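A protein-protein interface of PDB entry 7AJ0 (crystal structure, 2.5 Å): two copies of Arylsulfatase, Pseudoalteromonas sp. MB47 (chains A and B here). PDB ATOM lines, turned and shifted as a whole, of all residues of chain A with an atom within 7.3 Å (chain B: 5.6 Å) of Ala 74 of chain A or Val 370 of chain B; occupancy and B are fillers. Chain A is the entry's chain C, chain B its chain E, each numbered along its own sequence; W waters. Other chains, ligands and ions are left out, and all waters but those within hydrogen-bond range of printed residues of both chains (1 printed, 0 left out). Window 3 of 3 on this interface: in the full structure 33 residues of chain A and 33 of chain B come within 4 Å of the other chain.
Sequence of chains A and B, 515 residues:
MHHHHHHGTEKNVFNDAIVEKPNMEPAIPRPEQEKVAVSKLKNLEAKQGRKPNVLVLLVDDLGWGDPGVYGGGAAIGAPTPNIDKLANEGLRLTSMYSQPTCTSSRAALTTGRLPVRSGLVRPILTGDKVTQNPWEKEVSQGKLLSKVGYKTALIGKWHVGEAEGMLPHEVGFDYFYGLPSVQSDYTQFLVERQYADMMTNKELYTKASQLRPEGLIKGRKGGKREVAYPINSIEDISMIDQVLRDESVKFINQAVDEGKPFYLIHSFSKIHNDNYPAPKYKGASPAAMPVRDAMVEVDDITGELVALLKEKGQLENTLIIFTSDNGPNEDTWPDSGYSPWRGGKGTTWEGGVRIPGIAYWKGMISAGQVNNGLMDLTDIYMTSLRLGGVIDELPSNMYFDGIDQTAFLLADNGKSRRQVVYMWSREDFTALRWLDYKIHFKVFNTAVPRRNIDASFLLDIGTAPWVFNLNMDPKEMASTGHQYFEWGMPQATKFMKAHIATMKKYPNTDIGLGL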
ATOM      1  N   ASP A  66      17.718  11.825 -22.791  1.00  0.00           N
ATOM      2  CA  ASP A  66      16.790  12.920 -22.513  1.00  0.00           C
ATOM      3  C   ASP A  66      15.359  12.559 -22.886  1.00  0.00           C
ATOM      4  O   ASP A  66      14.451  12.805 -22.073  1.00  0.00           O
ATOM      5  CB  ASP A  66      17.257  14.193 -23.224  1.00  0.00           C
ATOM      6  CG  ASP A  66      18.241  15.005 -22.388  1.00  0.00           C
ATOM      7  OD1 ASP A  66      17.946  15.260 -21.200  1.00  0.00           O
ATOM      8  OD2 ASP A  66      19.310  15.385 -22.918  1.00  0.00           O
ATOM      9  N   PRO A  67      15.079  11.986 -24.056  1.00  0.00           N
ATOM     10  CA  PRO A  67      13.691  11.638 -24.386  1.00  0.00           C
ATOM     11  C   PRO A  67      13.163  10.518 -23.504  1.00  0.00           C
ATOM     12  O   PRO A  67      13.914   9.665 -23.023  1.00  0.00           O
ATOM     13  CB  PRO A  67      13.766  11.198 -25.854  1.00  0.00           C
ATOM     14  CG  PRO A  67      15.092  11.691 -26.357  1.00  0.00           C
ATOM     15  CD  PRO A  67      16.003  11.693 -25.166  1.00  0.00           C
ATOM     16  N   GLY A  68      11.841  10.520 -23.315  1.00  0.00           N
ATOM     17  CA  GLY A  68      11.226   9.545 -22.429  1.00  0.00           C
ATOM     18  C   GLY A  68      11.421   8.111 -22.884  1.00  0.00           C
ATOM     19  O   GLY A  68      11.658   7.218 -22.066  1.00  0.00           O
ATOM     20  N   GLY A  71      14.587   6.406 -21.620  1.00  0.00           N
ATOM     21  CA  GLY A  71      14.809   6.343 -20.193  1.00  0.00           C
ATOM     22  C   GLY A  71      14.865   7.674 -19.479  1.00  0.00           C
ATOM     23  O   GLY A  71      15.279   7.712 -18.313  1.00  0.00           O
ATOM     24  N   GLY A  72      14.473   8.762 -20.136  1.00  0.00           N
ATOM     25  CA  GLY A  72      14.437  10.063 -19.499  1.00  0.00           C
ATOM     26  C   GLY A  72      13.024  10.577 -19.319  1.00  0.00           C
ATOM     27  O   GLY A  72      12.228   9.980 -18.586  1.00  0.00           O
ATOM     28  N   GLY A  73      12.702  11.680 -19.986  1.00  0.00           N
ATOM     29  CA  GLY A  73      11.366  12.237 -19.942  1.00  0.00           C
ATOM     30  C   GLY A  73      10.860  12.484 -18.538  1.00  0.00           C
ATOM     31  O   GLY A  73      11.464  13.243 -17.776  1.00  0.00           O
ATOM     32  N   ALA A  74       9.746  11.843 -18.181  1.00  0.00           N
ATOM     33  CA  ALA A  74       9.167  12.055 -16.861  1.00  0.00           C
ATOM     34  C   ALA A  74      10.115  11.649 -15.741  1.00  0.00           C
ATOM     35  O   ALA A  74       9.941  12.102 -14.605  1.00  0.00           O
ATOM     36  CB  ALA A  74       7.852  11.283 -16.738  1.00  0.00           C
ATOM     37  N   ALA A  75      11.116  10.815 -16.031  1.00  0.00           N
ATOM     38  CA  ALA A  75      12.053  10.394 -14.998  1.00  0.00           C
ATOM     39  C   ALA A  75      12.992  11.513 -14.569  1.00  0.00           C
ATOM     40  O   ALA A  75      13.550  11.444 -13.468  1.00  0.00           O
ATOM     41  CB  ALA A  75      12.873   9.197 -15.486  1.00  0.00           C
ATOM     42  N   ILE A  76      13.180  12.535 -15.406  1.00  0.00           N
ATOM     43  CA  ILE A  76      14.034  13.668 -15.081  1.00  0.00           C
ATOM     44  C   ILE A  76      13.272  14.991 -15.174  1.00  0.00           C
ATOM     45  O   ILE A  76      13.879  16.049 -15.299  1.00  0.00           O
ATOM     46  CB  ILE A  76      15.289  13.692 -15.976  1.00  0.00           C
ATOM     47  CG1 ILE A  76      14.890  13.737 -17.453  1.00  0.00           C
ATOM     48  CG2 ILE A  76      16.165  12.482 -15.684  1.00  0.00           C
ATOM     49  CD1 ILE A  76      16.036  14.083 -18.378  1.00  0.00           C
ATOM     50  N   GLY A  77      11.945  14.941 -15.128  1.00  0.00           N
ATOM     51  CA  GLY A  77      11.159  16.150 -15.028  1.00  0.00           C
ATOM     52  C   GLY A  77      10.960  16.916 -16.309  1.00  0.00           C
ATOM     53  O   GLY A  77      10.830  18.145 -16.274  1.00  0.00           O
ATOM     54  N   ALA A  78      10.910  16.244 -17.450  1.00  0.00           N
ATOM     55  CA  ALA A  78      10.617  16.892 -18.737  1.00  0.00           C
ATOM     56  C   ALA A  78      10.041  15.890 -19.709  1.00  0.00           C
ATOM     57  O   ALA A  78      10.705  15.425 -20.634  1.00  0.00           O
ATOM     58  CB  ALA A  78      11.875  17.542 -19.317  1.00  0.00           C
ATOM     59  N   PRO A  79       8.759  15.542 -19.537  1.00  0.00           N
ATOM     60  CA  PRO A  79       8.144  14.580 -20.469  1.00  0.00           C
ATOM     61  C   PRO A  79       8.171  15.093 -21.903  1.00  0.00           C
ATOM     62  O   PRO A  79       7.993  16.286 -22.161  1.00  0.00           O
ATOM     63  CB  PRO A  79       6.705  14.433 -19.949  1.00  0.00           C
ATOM     64  CG  PRO A  79       6.480  15.626 -19.068  1.00  0.00           C
ATOM     65  CD  PRO A  79       7.820  15.967 -18.481  1.00  0.00           C
ATOM     66  N   THR A  80       8.411  14.175 -22.838  1.00  0.00           N
ATOM     67  CA  THR A  80       8.507  14.485 -24.264  1.00  0.00           C
ATOM     68  C   THR A  80       7.522  13.607 -25.026  1.00  0.00           C
ATOM     69  O   THR A  80       7.915  12.671 -25.731  1.00  0.00           O
ATOM     70  CB  THR A  80       9.934  14.278 -24.778  1.00  0.00           C
ATOM     71  OG1 THR A  80      10.309  12.901 -24.630  1.00  0.00           O
ATOM     72  CG2 THR A  80      10.919  15.153 -24.006  1.00  0.00           C
ATOM     73  N   ASP A  84       8.377  11.093 -28.032  1.00  0.00           N
ATOM     74  CA  ASP A  84       8.089   9.710 -27.664  1.00  0.00           C
ATOM     75  C   ASP A  84       7.175   9.046 -28.689  1.00  0.00           C
ATOM     76  O   ASP A  84       7.412   7.908 -29.108  1.00  0.00           O
ATOM     77  CB  ASP A  84       7.449   9.658 -26.274  1.00  0.00           C
ATOM     78  CG  ASP A  84       8.441   9.931 -25.153  1.00  0.00           C
ATOM     79  OD1 ASP A  84       9.642  10.135 -25.438  1.00  0.00           O
ATOM     80  OD2 ASP A  84       8.011   9.937 -23.979  1.00  0.00           O
ATOM     81  N   PRO A 286       7.948  19.784 -15.026  1.00  0.00           N
ATOM     82  CA  PRO A 286       7.905  19.501 -13.580  1.00  0.00           C
ATOM     83  C   PRO A 286       9.188  19.891 -12.867  1.00  0.00           C
ATOM     84  O   PRO A 286       9.144  20.371 -11.729  1.00  0.00           O
ATOM     85  CB  PRO A 286       7.653  17.987 -13.524  1.00  0.00           C
ATOM     86  CG  PRO A 286       6.978  17.666 -14.822  1.00  0.00           C
ATOM     87  CD  PRO A 286       7.564  18.613 -15.838  1.00  0.00           C
ATOM     88  N   LEU B  91       1.099   1.240 -16.851  1.00  0.00           N
ATOM     89  CA  LEU B  91       1.633   2.367 -16.095  1.00  0.00           C
ATOM     90  C   LEU B  91       3.085   2.093 -15.738  1.00  0.00           C
ATOM     91  O   LEU B  91       3.381   1.142 -15.006  1.00  0.00           O
ATOM     92  CB  LEU B  91       0.800   2.601 -14.832  1.00  0.00           C
ATOM     93  CG  LEU B  91       1.370   3.519 -13.753  1.00  0.00           C
ATOM     94  CD1 LEU B  91       1.604   4.914 -14.295  1.00  0.00           C
ATOM     95  CD2 LEU B  91       0.434   3.555 -12.551  1.00  0.00           C
ATOM     96  N   ARG B  92       3.987   2.931 -16.246  1.00  0.00           N
ATOM     97  CA  ARG B  92       5.411   2.822 -15.960  1.00  0.00           C
ATOM     98  C   ARG B  92       5.781   3.822 -14.870  1.00  0.00           C
ATOM     99  O   ARG B  92       5.628   5.033 -15.057  1.00  0.00           O
ATOM    100  CB  ARG B  92       6.243   3.066 -17.220  1.00  0.00           C
ATOM    101  CG  ARG B  92       7.740   2.910 -17.004  1.00  0.00           C
ATOM    102  CD  ARG B  92       8.483   2.643 -18.305  1.00  0.00           C
ATOM    103  NE  ARG B  92       8.403   3.752 -19.255  1.00  0.00           N
ATOM    104  CZ  ARG B  92       9.241   4.787 -19.279  1.00  0.00           C
ATOM    105  NH1 ARG B  92      10.227   4.872 -18.395  1.00  0.00           N
ATOM    106  NH2 ARG B  92       9.091   5.741 -20.188  1.00  0.00           N
ATOM    107  N   THR B  94       8.598   5.657 -12.751  1.00  0.00           N
ATOM    108  CA  THR B  94      10.001   6.025 -12.868  1.00  0.00           C
ATOM    109  C   THR B  94      10.631   6.396 -11.532  1.00  0.00           C
ATOM    110  O   THR B  94      11.810   6.765 -11.500  1.00  0.00           O
ATOM    111  CB  THR B  94      10.164   7.188 -13.858  1.00  0.00           C
ATOM    112  OG1 THR B  94       9.295   8.266 -13.485  1.00  0.00           O
ATOM    113  CG2 THR B  94       9.836   6.739 -15.280  1.00  0.00           C
ATOM    114  N   GLY B 368      -0.220   3.615 -21.575  1.00  0.00           N
ATOM    115  CA  GLY B 368       0.671   4.675 -21.996  1.00  0.00           C
ATOM    116  C   GLY B 368       0.984   5.728 -20.961  1.00  0.00           C
ATOM    117  O   GLY B 368       1.325   6.859 -21.324  1.00  0.00           O
ATOM    118  N   GLN B 369       0.887   5.392 -19.678  1.00  0.00           N
ATOM    119  CA  GLN B 369       1.205   6.337 -18.621  1.00  0.00           C
ATOM    120  C   GLN B 369       2.649   6.177 -18.169  1.00  0.00           C
ATOM    121  O   GLN B 369       3.150   5.057 -18.026  1.00  0.00           O
ATOM    122  CB  GLN B 369       0.287   6.139 -17.417  1.00  0.00           C
ATOM    123  CG  GLN B 369      -1.149   6.510 -17.647  1.00  0.00           C
ATOM    124  CD  GLN B 369      -1.993   6.239 -16.426  1.00  0.00           C
ATOM    125  OE1 GLN B 369      -2.033   7.043 -15.494  1.00  0.00           O
ATOM    126  NE2 GLN B 369      -2.655   5.086 -16.409  1.00  0.00           N
ATOM    127  N   VAL B 370       3.311   7.306 -17.936  1.00  0.00           N
ATOM    128  CA  VAL B 370       4.626   7.349 -17.308  1.00  0.00           C
ATOM    129  C   VAL B 370       4.527   8.341 -16.156  1.00  0.00           C
ATOM    130  O   VAL B 370       4.249   9.526 -16.376  1.00  0.00           O
ATOM    131  CB  VAL B 370       5.730   7.755 -18.295  1.00  0.00           C
ATOM    132  CG1 VAL B 370       7.096   7.648 -17.637  1.00  0.00           C
ATOM    133  CG2 VAL B 370       5.671   6.886 -19.543  1.00  0.00           C
ATOM    134  N   ASN B 371       4.744   7.857 -14.933  1.00  0.00           N
ATOM    135  CA  ASN B 371       4.470   8.622 -13.723  1.00  0.00           C
ATOM    136  C   ASN B 371       5.670   8.571 -12.794  1.00  0.00           C
ATOM    137  O   ASN B 371       6.139   7.486 -12.438  1.00  0.00           O
ATOM    138  CB  ASN B 371       3.225   8.069 -13.020  1.00  0.00           C
ATOM    139  CG  ASN B 371       2.656   9.026 -11.999  1.00  0.00           C
ATOM    140  OD1 ASN B 371       3.380   9.572 -11.166  1.00  0.00           O
ATOM    141  ND2 ASN B 371       1.348   9.240 -12.060  1.00  0.00           N
ATOM    142  N   ASN B 372       6.153   9.748 -12.391  1.00  0.00           N
ATOM    143  CA  ASN B 372       7.332   9.867 -11.546  1.00  0.00           C
ATOM    144  C   ASN B 372       6.982   9.998 -10.065  1.00  0.00           C
ATOM    145  O   ASN B 372       7.825  10.426  -9.269  1.00  0.00           O
ATOM    146  CB  ASN B 372       8.178  11.062 -11.990  1.00  0.00           C
ATOM    147  CG  ASN B 372       9.647  10.904 -11.637  1.00  0.00           C
ATOM    148  OD1 ASN B 372      10.202   9.810 -11.724  1.00  0.00           O
ATOM    149  ND2 ASN B 372      10.281  11.997 -11.233  1.00  0.00           N
ATOM    150  N   ASN B 413      -2.824   9.627 -14.788  1.00  0.00           N
ATOM    151  CA  ASN B 413      -1.763  10.570 -14.445  1.00  0.00           C
ATOM    152  C   ASN B 413      -1.960  11.106 -13.033  1.00  0.00           C
ATOM    153  O   ASN B 413      -1.785  12.295 -12.761  1.00  0.00           O
ATOM    154  CB  ASN B 413      -1.701  11.707 -15.460  1.00  0.00           C
ATOM    155  CG  ASN B 413      -1.595  11.202 -16.881  1.00  0.00           C
ATOM    156  OD1 ASN B 413      -0.551  10.694 -17.294  1.00  0.00           O
ATOM    157  ND2 ASN B 413      -2.679  11.329 -17.637  1.00  0.00           N
ATOM    158  N   ASN B 471      16.093  15.486 -10.640  1.00  0.00           N
ATOM    159  CA  ASN B 471      15.739  15.892 -11.996  1.00  0.00           C
ATOM    160  C   ASN B 471      16.953  16.446 -12.730  1.00  0.00           C
ATOM    161  O   ASN B 471      17.139  16.187 -13.924  1.00  0.00           O
ATOM    162  CB  ASN B 471      14.625  16.938 -11.973  1.00  0.00           C
ATOM    163  CG  ASN B 471      13.299  16.368 -11.525  1.00  0.00           C
ATOM    164  OD1 ASN B 471      12.962  15.222 -11.825  1.00  0.00           O
ATOM    165  ND2 ASN B 471      12.533  17.171 -10.799  1.00  0.00           N
HETATM  166  O   HOH W   1       8.049   7.903 -22.184  1.00  0.00           O
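The backbone carbonyl oxygen (O) of Ala 74 of chain A sits close to the side-chain amide nitrogen (ND2) of Asn 372 of chain B (3.4 Å).
N of Gly 77 of chain A sits at hydrogen-bond distance from OD1 of Asn 471 of chain B (3.5 Å).
No position is printed for both chains.
Of the 7 pairs that touch across the chains among the printed residues, none has its exchanged pair printed and touching as well.
Water W1 lies within hydrogen-bond range of the side-chain carboxylate of Asp 84 of chain A (2.7 Å) and the guanidinium group of Arg 92 of chain B (3.1 Å).
Of chain B, only Val 370 and Asn 372 come within 4 Å of Ala 74 of chain A.
Val 370 of chain B touches one residue of chain A.
Printed residues of chain A within 4 Å of Thr 94 of chain B: Ala 75.
Of the printed residues of chain B, Gly 68 of chain A touches Arg 92 (3.5 Å).
Of the printed residues of chain A, Asn 471 of chain B touches Ile 76 and Gly 77.
Printed residues of chain A within 4 Å of Asn 372 of chain B: Ala 74 and Ala 75.
Of the printed residues of chain A, Arg 92 of chain B touches Gly 68.
Asp 66 of chain A touches none of the printed residues of chain B.
The nearest residue of chain A that does not touch Val 370 of chain B is Ala 75 of chain A (5.4 Å).
The nearest printed residue of chain B that does not touch Ile 76 of chain A is Asn 372 of chain B (5.1 Å).
Hydrophobic or aromatic side chains of chain B that line the printed part of chain A: Val 370.
Of the 15 printed residues of chain A, 5 touch a printed residue of chain B.
Printed residues of chain A that touch a printed residue of chain B: Gly 68, Ala 74, Ala 75, Ile 76 and Gly 77.
Among the printed residues, merely in contact across the chains: Ile 76 of chain A with Asn 471 of chain B, Gly 68 of chain A with Arg 92 of chain B, Ala 75 of chain A with Thr 94 of chain B, Ala 75 of chain A with Asn 372 of chain B and Ala 74 of chain A with Val 370 of chain B.
N of Gly 68 of chain A sits at hydrogen-bond distance from OG1 of Thr 80 of chain A.
The side-chain carboxylate of Asp 84 of chain A sits at hydrogen-bond distance from the backbone NH of Gly 68 of chain A (3.1 Å).
The backbone NH (N) of Arg 92 of chain B is in hydrogen-bond range of the backbone carbonyl oxygen (O) of Gln 369 of chain B (2.9 Å).
N of Asn 371 of chain B sits at hydrogen-bond distance from O of Arg 92 of chain B (3.0 Å).
The backbone NH (N) of Thr 94 of chain B lies within hydrogen-bond range of the backbone carbonyl oxygen (O) of Asn 371 of chain B, at 3.1 Å.
The side-chain hydroxyl of Thr 94 of chain B lies within hydrogen-bond range of the side-chain amide oxygen of Asn 372 of chain B (2.5 Å).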
